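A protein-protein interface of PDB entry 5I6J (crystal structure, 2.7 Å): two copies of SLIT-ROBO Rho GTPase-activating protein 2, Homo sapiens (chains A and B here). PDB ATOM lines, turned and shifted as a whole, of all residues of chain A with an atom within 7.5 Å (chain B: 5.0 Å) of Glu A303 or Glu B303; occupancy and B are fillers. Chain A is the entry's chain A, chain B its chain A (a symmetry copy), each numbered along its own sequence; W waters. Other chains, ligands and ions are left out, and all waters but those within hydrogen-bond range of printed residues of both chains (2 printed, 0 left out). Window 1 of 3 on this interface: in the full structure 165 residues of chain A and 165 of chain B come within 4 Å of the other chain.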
ATOM      1  N   ASP A 112      29.676   4.561 -17.732  1.00  0.00           N
ATOM      2  CA  ASP A 112      29.497   5.898 -18.307  1.00  0.00           C
ATOM      3  C   ASP A 112      30.765   6.740 -18.326  1.00  0.00           C
ATOM      4  O   ASP A 112      30.994   7.511 -19.229  1.00  0.00           O
ATOM      5  CB  ASP A 112      28.432   6.679 -17.552  1.00  0.00           C
ATOM      6  CG  ASP A 112      27.024   6.131 -17.748  1.00  0.00           C
ATOM      7  OD1 ASP A 112      26.829   5.217 -18.620  1.00  0.00           O
ATOM      8  OD2 ASP A 112      26.126   6.629 -16.975  1.00  0.00           O
ATOM      9  N   LEU A 116      33.023   8.264 -21.344  1.00  0.00           N
ATOM     10  CA  LEU A 116      33.388   9.661 -21.443  1.00  0.00           C
ATOM     11  C   LEU A 116      34.891   9.827 -21.708  1.00  0.00           C
ATOM     12  O   LEU A 116      35.361  10.863 -22.211  1.00  0.00           O
ATOM     13  CB  LEU A 116      33.027  10.290 -20.129  1.00  0.00           C
ATOM     14  CG  LEU A 116      32.632  11.720 -20.123  1.00  0.00           C
ATOM     15  CD1 LEU A 116      31.136  11.673 -20.269  1.00  0.00           C
ATOM     16  CD2 LEU A 116      33.027  12.177 -18.742  1.00  0.00           C
ATOM     17  N   LEU A 296      29.495  18.904 -24.286  1.00  0.00           N
ATOM     18  CA  LEU A 296      28.120  19.062 -23.762  1.00  0.00           C
ATOM     19  C   LEU A 296      27.215  17.873 -24.120  1.00  0.00           C
ATOM     20  O   LEU A 296      26.461  17.397 -23.307  1.00  0.00           O
ATOM     21  CB  LEU A 296      27.523  20.360 -24.241  1.00  0.00           C
ATOM     22  CG  LEU A 296      28.360  21.500 -23.692  1.00  0.00           C
ATOM     23  CD1 LEU A 296      27.999  22.819 -24.367  1.00  0.00           C
ATOM     24  CD2 LEU A 296      28.109  21.591 -22.179  1.00  0.00           C
ATOM     25  N   SER A 297      27.338  17.341 -25.321  1.00  0.00           N
ATOM     26  CA  SER A 297      26.578  16.159 -25.655  1.00  0.00           C
ATOM     27  C   SER A 297      26.840  15.055 -24.646  1.00  0.00           C
ATOM     28  O   SER A 297      25.881  14.543 -24.048  1.00  0.00           O
ATOM     29  CB  SER A 297      26.854  15.644 -27.077  1.00  0.00           C
ATOM     30  OG  SER A 297      26.182  14.398 -27.163  1.00  0.00           O
ATOM     31  N   ALA A 298      28.132  14.727 -24.463  1.00  0.00           N
ATOM     32  CA  ALA A 298      28.597  13.649 -23.606  1.00  0.00           C
ATOM     33  C   ALA A 298      28.185  13.854 -22.164  1.00  0.00           C
ATOM     34  O   ALA A 298      27.686  12.930 -21.543  1.00  0.00           O
ATOM     35  CB  ALA A 298      30.095  13.577 -23.676  1.00  0.00           C
ATOM     36  N   GLU A 299      28.407  15.054 -21.631  1.00  0.00           N
ATOM     37  CA  GLU A 299      27.860  15.421 -20.332  1.00  0.00           C
ATOM     38  C   GLU A 299      26.336  15.240 -20.151  1.00  0.00           C
ATOM     39  O   GLU A 299      25.903  14.773 -19.093  1.00  0.00           O
ATOM     40  CB  GLU A 299      28.244  16.856 -19.966  1.00  0.00           C
ATOM     41  CG  GLU A 299      29.672  17.028 -19.528  1.00  0.00           C
ATOM     42  CD  GLU A 299      30.128  15.950 -18.544  1.00  0.00           C
ATOM     43  OE1 GLU A 299      31.116  15.257 -18.910  1.00  0.00           O
ATOM     44  OE2 GLU A 299      29.507  15.792 -17.435  1.00  0.00           O
ATOM     45  N   LEU A 300      25.531  15.630 -21.149  1.00  0.00           N
ATOM     46  CA  LEU A 300      24.087  15.407 -21.091  1.00  0.00           C
ATOM     47  C   LEU A 300      23.726  13.907 -21.055  1.00  0.00           C
ATOM     48  O   LEU A 300      22.817  13.501 -20.331  1.00  0.00           O
ATOM     49  CB  LEU A 300      23.352  16.154 -22.214  1.00  0.00           C
ATOM     50  CG  LEU A 300      21.821  15.990 -22.412  1.00  0.00           C
ATOM     51  CD1 LEU A 300      21.040  17.308 -22.377  1.00  0.00           C
ATOM     52  CD2 LEU A 300      21.527  15.233 -23.705  1.00  0.00           C
ATOM     53  N   ASN A 301      24.403  13.073 -21.824  1.00  0.00           N
ATOM     54  CA  ASN A 301      24.060  11.659 -21.734  1.00  0.00           C
ATOM     55  C   ASN A 301      24.455  11.006 -20.424  1.00  0.00           C
ATOM     56  O   ASN A 301      23.884   9.990 -20.060  1.00  0.00           O
ATOM     57  CB  ASN A 301      24.638  10.855 -22.874  1.00  0.00           C
ATOM     58  CG  ASN A 301      23.929  11.112 -24.152  1.00  0.00           C
ATOM     59  OD1 ASN A 301      23.079  10.317 -24.589  1.00  0.00           O
ATOM     60  ND2 ASN A 301      24.264  12.226 -24.772  1.00  0.00           N
ATOM     61  N   LEU A 302      25.458  11.551 -19.743  1.00  0.00           N
ATOM     62  CA  LEU A 302      25.856  11.021 -18.461  1.00  0.00           C
ATOM     63  C   LEU A 302      24.717  11.394 -17.492  1.00  0.00           C
ATOM     64  O   LEU A 302      24.037  10.497 -16.969  1.00  0.00           O
ATOM     65  CB  LEU A 302      27.200  11.615 -18.065  1.00  0.00           C
ATOM     66  CG  LEU A 302      28.116  11.013 -16.999  1.00  0.00           C
ATOM     67  CD1 LEU A 302      28.984   9.912 -17.567  1.00  0.00           C
ATOM     68  CD2 LEU A 302      29.015  12.125 -16.493  1.00  0.00           C
ATOM     69  N   GLU A 303      24.467  12.698 -17.325  1.00  0.00           N
ATOM     70  CA  GLU A 303      23.272  13.199 -16.628  1.00  0.00           C
ATOM     71  C   GLU A 303      22.091  12.256 -16.804  1.00  0.00           C
ATOM     72  O   GLU A 303      21.598  11.703 -15.849  1.00  0.00           O
ATOM     73  CB  GLU A 303      22.880  14.623 -17.091  1.00  0.00           C
ATOM     74  CG  GLU A 303      21.569  15.171 -16.483  1.00  0.00           C
ATOM     75  CD  GLU A 303      21.359  16.672 -16.696  1.00  0.00           C
ATOM     76  OE1 GLU A 303      20.590  17.278 -15.904  1.00  0.00           O
ATOM     77  OE2 GLU A 303      21.965  17.240 -17.639  1.00  0.00           O
ATOM     78  N   GLN A 304      21.640  12.071 -18.043  1.00  0.00           N
ATOM     79  CA  GLN A 304      20.487  11.204 -18.293  1.00  0.00           C
ATOM     80  C   GLN A 304      20.641   9.778 -17.803  1.00  0.00           C
ATOM     81  O   GLN A 304      19.787   9.273 -17.118  1.00  0.00           O
ATOM     82  CB  GLN A 304      20.153  11.156 -19.738  1.00  0.00           C
ATOM     83  CG  GLN A 304      19.541  12.430 -20.260  1.00  0.00           C
ATOM     84  CD  GLN A 304      19.156  12.280 -21.730  1.00  0.00           C
ATOM     85  OE1 GLN A 304      19.010  13.279 -22.437  1.00  0.00           O
ATOM     86  NE2 GLN A 304      18.991  11.018 -22.199  1.00  0.00           N
ATOM     87  N   SER A 305      21.750   9.138 -18.116  1.00  0.00           N
ATOM     88  CA  SER A 305      22.021   7.782 -17.653  1.00  0.00           C
ATOM     89  C   SER A 305      21.990   7.664 -16.128  1.00  0.00           C
ATOM     90  O   SER A 305      21.414   6.688 -15.591  1.00  0.00           O
ATOM     91  CB  SER A 305      23.353   7.328 -18.188  1.00  0.00           C
ATOM     92  OG  SER A 305      23.715   6.143 -17.526  1.00  0.00           O
ATOM     93  N   LYS A 306      22.570   8.666 -15.451  1.00  0.00           N
ATOM     94  CA  LYS A 306      22.649   8.717 -13.989  1.00  0.00           C
ATOM     95  C   LYS A 306      21.241   8.830 -13.395  1.00  0.00           C
ATOM     96  O   LYS A 306      20.880   8.008 -12.556  1.00  0.00           O
ATOM     97  CB  LYS A 306      23.575   9.861 -13.525  1.00  0.00           C
ATOM     98  CG  LYS A 306      24.253   9.610 -12.189  1.00  0.00           C
ATOM     99  CD  LYS A 306      24.423  10.903 -11.401  1.00  0.00           C
ATOM    100  CE  LYS A 306      25.835  11.469 -11.496  1.00  0.00           C
ATOM    101  NZ  LYS A 306      26.557  11.169 -10.234  1.00  0.00           N
ATOM    102  N   HIS A 307      20.458   9.813 -13.867  1.00  0.00           N
ATOM    103  CA  HIS A 307      19.042   9.993 -13.559  1.00  0.00           C
ATOM    104  C   HIS A 307      18.183   8.735 -13.653  1.00  0.00           C
ATOM    105  O   HIS A 307      17.467   8.437 -12.717  1.00  0.00           O
ATOM    106  CB  HIS A 307      18.461  11.064 -14.450  1.00  0.00           C
ATOM    107  CG  HIS A 307      17.207  11.683 -13.923  1.00  0.00           C
ATOM    108  ND1 HIS A 307      17.191  12.920 -13.310  1.00  0.00           N
ATOM    109  CD2 HIS A 307      15.917  11.274 -13.975  1.00  0.00           C
ATOM    110  CE1 HIS A 307      15.950  13.234 -12.980  1.00  0.00           C
ATOM    111  NE2 HIS A 307      15.157  12.255 -13.379  1.00  0.00           N
ATOM    112  N   GLU A 308      18.253   7.994 -14.749  1.00  0.00           N
ATOM    113  CA  GLU A 308      17.585   6.665 -14.878  1.00  0.00           C
ATOM    114  C   GLU A 308      17.978   5.721 -13.731  1.00  0.00           C
ATOM    115  O   GLU A 308      17.138   5.015 -13.207  1.00  0.00           O
ATOM    116  CB  GLU A 308      17.955   5.984 -16.213  1.00  0.00           C
ATOM    117  CG  GLU A 308      16.809   5.246 -16.920  1.00  0.00           C
ATOM    118  CD  GLU A 308      17.223   4.037 -17.807  1.00  0.00           C
ATOM    119  OE1 GLU A 308      18.426   3.702 -17.945  1.00  0.00           O
ATOM    120  OE2 GLU A 308      16.316   3.383 -18.380  1.00  0.00           O
ATOM    121  N   GLY A 309      19.261   5.708 -13.362  1.00  0.00           N
ATOM    122  CA  GLY A 309      19.765   4.882 -12.282  1.00  0.00           C
ATOM    123  C   GLY A 309      19.161   5.308 -10.966  1.00  0.00           C
ATOM    124  O   GLY A 309      18.537   4.489 -10.292  1.00  0.00           O
ATOM    125  N   LEU A 310      19.292   6.588 -10.602  1.00  0.00           N
ATOM    126  CA  LEU A 310      18.836   7.045  -9.287  1.00  0.00           C
ATOM    127  C   LEU A 310      17.328   6.926  -9.108  1.00  0.00           C
ATOM    128  O   LEU A 310      16.835   6.858  -7.964  1.00  0.00           O
ATOM    129  CB  LEU A 310      19.217   8.471  -9.023  1.00  0.00           C
ATOM    130  CG  LEU A 310      20.659   8.892  -8.968  1.00  0.00           C
ATOM    131  CD1 LEU A 310      20.733  10.413  -8.985  1.00  0.00           C
ATOM    132  CD2 LEU A 310      21.354   8.332  -7.743  1.00  0.00           C
ATOM    133  N   PHE A 413      25.169  22.303  -0.286  1.00  0.00           N
ATOM    134  CA  PHE A 413      25.701  22.720  -1.578  1.00  0.00           C
ATOM    135  C   PHE A 413      25.553  24.234  -1.732  1.00  0.00           C
ATOM    136  O   PHE A 413      25.688  24.759  -2.837  1.00  0.00           O
ATOM    137  CB  PHE A 413      25.022  21.951  -2.737  1.00  0.00           C
ATOM    138  CG  PHE A 413      25.261  20.453  -2.721  1.00  0.00           C
ATOM    139  CD1 PHE A 413      24.501  19.595  -1.898  1.00  0.00           C
ATOM    140  CD2 PHE A 413      26.244  19.876  -3.539  1.00  0.00           C
ATOM    141  CE1 PHE A 413      24.720  18.201  -1.896  1.00  0.00           C
ATOM    142  CE2 PHE A 413      26.454  18.485  -3.551  1.00  0.00           C
ATOM    143  CZ  PHE A 413      25.690  17.651  -2.732  1.00  0.00           C
ATOM    144  N   GLU B 299      22.798  13.400  -4.352  1.00  0.00           N
ATOM    145  CA  GLU B 299      22.844  13.214  -5.796  1.00  0.00           C
ATOM    146  C   GLU B 299      22.057  14.237  -6.647  1.00  0.00           C
ATOM    147  O   GLU B 299      22.562  14.677  -7.684  1.00  0.00           O
ATOM    148  CB  GLU B 299      22.407  11.799  -6.178  1.00  0.00           C
ATOM    149  CG  GLU B 299      23.433  10.733  -5.905  1.00  0.00           C
ATOM    150  CD  GLU B 299      24.840  11.134  -6.349  1.00  0.00           C
ATOM    151  OE1 GLU B 299      25.717  11.148  -5.441  1.00  0.00           O
ATOM    152  OE2 GLU B 299      25.064  11.436  -7.573  1.00  0.00           O
ATOM    153  N   LEU B 300      20.829  14.586  -6.238  1.00  0.00           N
ATOM    154  CA  LEU B 300      20.060  15.614  -6.937  1.00  0.00           C
ATOM    155  C   LEU B 300      20.742  16.997  -6.880  1.00  0.00           C
ATOM    156  O   LEU B 300      20.745  17.734  -7.867  1.00  0.00           O
ATOM    157  CB  LEU B 300      18.605  15.665  -6.449  1.00  0.00           C
ATOM    158  CG  LEU B 300      17.623  16.744  -6.979  1.00  0.00           C
ATOM    159  CD1 LEU B 300      16.348  16.174  -7.611  1.00  0.00           C
ATOM    160  CD2 LEU B 300      17.270  17.736  -5.874  1.00  0.00           C
ATOM    161  N   ASN B 301      21.311  17.379  -5.750  1.00  0.00           N
ATOM    162  CA  ASN B 301      21.979  18.674  -5.746  1.00  0.00           C
ATOM    163  C   ASN B 301      23.249  18.722  -6.574  1.00  0.00           C
ATOM    164  O   ASN B 301      23.662  19.794  -6.983  1.00  0.00           O
ATOM    165  CB  ASN B 301      22.289  19.155  -4.348  1.00  0.00           C
ATOM    166  CG  ASN B 301      21.070  19.600  -3.629  1.00  0.00           C
ATOM    167  OD1 ASN B 301      20.789  20.806  -3.520  1.00  0.00           O
ATOM    168  ND2 ASN B 301      20.324  18.636  -3.129  1.00  0.00           N
ATOM    169  N   LEU B 302      23.894  17.577  -6.777  1.00  0.00           N
ATOM    170  CA  LEU B 302      25.077  17.531  -7.601  1.00  0.00           C
ATOM    171  C   LEU B 302      24.582  17.753  -9.043  1.00  0.00           C
ATOM    172  O   LEU B 302      24.931  18.771  -9.663  1.00  0.00           O
ATOM    173  CB  LEU B 302      25.777  16.193  -7.405  1.00  0.00           C
ATOM    174  CG  LEU B 302      27.235  15.932  -7.782  1.00  0.00           C
ATOM    175  CD1 LEU B 302      28.182  16.372  -6.688  1.00  0.00           C
ATOM    176  CD2 LEU B 302      27.389  14.436  -7.984  1.00  0.00           C
ATOM    177  N   GLU B 303      23.721  16.853  -9.532  1.00  0.00           N
ATOM    178  CA  GLU B 303      22.983  17.055 -10.789  1.00  0.00           C
ATOM    179  C   GLU B 303      22.703  18.531 -11.037  1.00  0.00           C
ATOM    180  O   GLU B 303      23.171  19.092 -11.999  1.00  0.00           O
ATOM    181  CB  GLU B 303      21.658  16.256 -10.825  1.00  0.00           C
ATOM    182  CG  GLU B 303      20.776  16.507 -12.067  1.00  0.00           C
ATOM    183  CD  GLU B 303      19.641  15.495 -12.245  1.00  0.00           C
ATOM    184  OE1 GLU B 303      19.160  15.344 -13.399  1.00  0.00           O
ATOM    185  OE2 GLU B 303      19.242  14.852 -11.242  1.00  0.00           O
ATOM    186  N   GLN B 304      21.933  19.160 -10.152  1.00  0.00           N
ATOM    187  CA  GLN B 304      21.590  20.572 -10.336  1.00  0.00           C
ATOM    188  C   GLN B 304      22.776  21.510 -10.437  1.00  0.00           C
ATOM    189  O   GLN B 304      22.854  22.297 -11.348  1.00  0.00           O
ATOM    190  CB  GLN B 304      20.715  21.059  -9.241  1.00  0.00           C
ATOM    191  CG  GLN B 304      19.310  20.520  -9.303  1.00  0.00           C
ATOM    192  CD  GLN B 304      18.451  21.122  -8.194  1.00  0.00           C
ATOM    193  OE1 GLN B 304      17.422  20.550  -7.827  1.00  0.00           O
ATOM    194  NE2 GLN B 304      18.876  22.289  -7.649  1.00  0.00           N
ATOM    195  N   SER B 305      23.723  21.401  -9.528  1.00  0.00           N
ATOM    196  CA  SER B 305      24.930  22.219  -9.563  1.00  0.00           C
ATOM    197  C   SER B 305      25.708  22.066 -10.871  1.00  0.00           C
ATOM    198  O   SER B 305      26.176  23.081 -11.439  1.00  0.00           O
ATOM    199  CB  SER B 305      25.805  21.871  -8.388  1.00  0.00           C
ATOM    200  OG  SER B 305      27.062  22.466  -8.581  1.00  0.00           O
ATOM    201  N   LYS B 306      25.804  20.818 -11.352  1.00  0.00           N
ATOM    202  CA  LYS B 306      26.522  20.477 -12.584  1.00  0.00           C
ATOM    203  C   LYS B 306      25.830  21.128 -13.786  1.00  0.00           C
ATOM    204  O   LYS B 306      26.489  21.841 -14.539  1.00  0.00           O
ATOM    205  CB  LYS B 306      26.655  18.947 -12.741  1.00  0.00           C
ATOM    206  CG  LYS B 306      27.879  18.506 -13.526  1.00  0.00           C
ATOM    207  CD  LYS B 306      27.589  17.256 -14.349  1.00  0.00           C
ATOM    208  CE  LYS B 306      28.115  15.985 -13.691  1.00  0.00           C
ATOM    209  NZ  LYS B 306      29.361  15.570 -14.383  1.00  0.00           N
ATOM    210  N   HIS B 307      24.513  20.909 -13.923  1.00  0.00           N
ATOM    211  CA  HIS B 307      23.639  21.563 -14.894  1.00  0.00           C
ATOM    212  C   HIS B 307      23.794  23.076 -15.005  1.00  0.00           C
ATOM    213  O   HIS B 307      23.957  23.576 -16.101  1.00  0.00           O
ATOM    214  CB  HIS B 307      22.199  21.226 -14.589  1.00  0.00           C
ATOM    215  CG  HIS B 307      21.272  21.401 -15.748  1.00  0.00           C
ATOM    216  ND1 HIS B 307      20.815  20.337 -16.499  1.00  0.00           N
ATOM    217  CD2 HIS B 307      20.662  22.502 -16.247  1.00  0.00           C
ATOM    218  CE1 HIS B 307      19.985  20.777 -17.429  1.00  0.00           C
ATOM    219  NE2 HIS B 307      19.869  22.086 -17.293  1.00  0.00           N
HETATM  220  O   HOH W   1      23.261  17.801 -14.448  1.00  0.00           O
HETATM  221  O   HOH W   2      21.262  13.084 -13.472  1.00  0.00           O
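Glu A299 touches Lys B306, and with the chains exchanged Lys A306 touches Glu B299. Glu A303 touches its own counterpart, Glu B303. Glu A303 touches His B307, and with the chains exchanged His A307 touches Glu B303. Positions printed for both chains: 299, 300, 301, 302, 303, 304, 305, 306 and 307. Of the 7 pairs that touch across the chains among the printed residues, 5 have their exchanged pair printed and touching as well.
Among the printed residues, pairs that only touch across the chains: Leu A310 with Glu B299 (3.6 Å) and Phe A413 with Asn B301 (3.3 Å).
Leu A302 touches none of the printed residues of chain B. Of the printed residues of chain A, Asn B301 touches Phe A413. Leu B302 touches none of the printed residues of chain A. Of the printed residues of chain A, Glu B303 touches Glu A303 (3.5 Å) and His A307 (3.1 Å). Of the printed residues of chain A, Lys B306 touches Glu A299. The nearest printed residue of chain A that does not touch Asn B301 is Leu A310 (7.7 Å).
Water W2 lies within hydrogen-bond range of the backbone carbonyl oxygen of Glu A303 (2.8 Å), the side-chain carboxylate of Glu B303 (3.1 Å) and the backbone NH of His A307 (3.4 Å). Water W1 lies within hydrogen-bond range of the backbone carbonyl oxygen (O) of Glu B303 (2.8 Å), the side-chain carboxylate (OE1) of Glu A303 (3.1 Å) and the backbone NH (N) of His B307 (3.4 Å).
A ring nitrogen (ND1) of His A307 is in hydrogen-bond range of the side-chain carboxylate of Glu B303. OE1 of Glu A303 lies close to OE1 of Glu B303, 3.5 Å away. The side-chain carboxylate of Glu A299 lies within salt-bridge range of the side-chain amino group of Lys B306. A ring nitrogen (ND1) of His B307 sits at hydrogen-bond distance from the side-chain carboxylate of Glu A303, at 3.1 Å. NZ of Lys A306 lies within salt-bridge range of OE2 of Glu B299.
Printed residues of chain B that touch a printed residue of chain A: Glu B299, Asn B301, Glu B303, Lys B306 and His B307. Hydrophobic or aromatic side chains of chain B that line the printed part of chain A: His B307. Of the 18 printed residues of chain A, 6 touch a printed residue of chain B. Hydrophobic or aromatic side chains of chain A within 4 Å of the printed part of chain B: His A307, Leu A310 and Phe A413. Among the printed residues, 7 pairs touch across the chains. Among the printed residues, Asp or Glu carboxylates within 4 Å of a Lys or Arg side-chain nitrogen of the other chain: Glu A299 with Lys B306 and Lys A306 with Glu B299.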
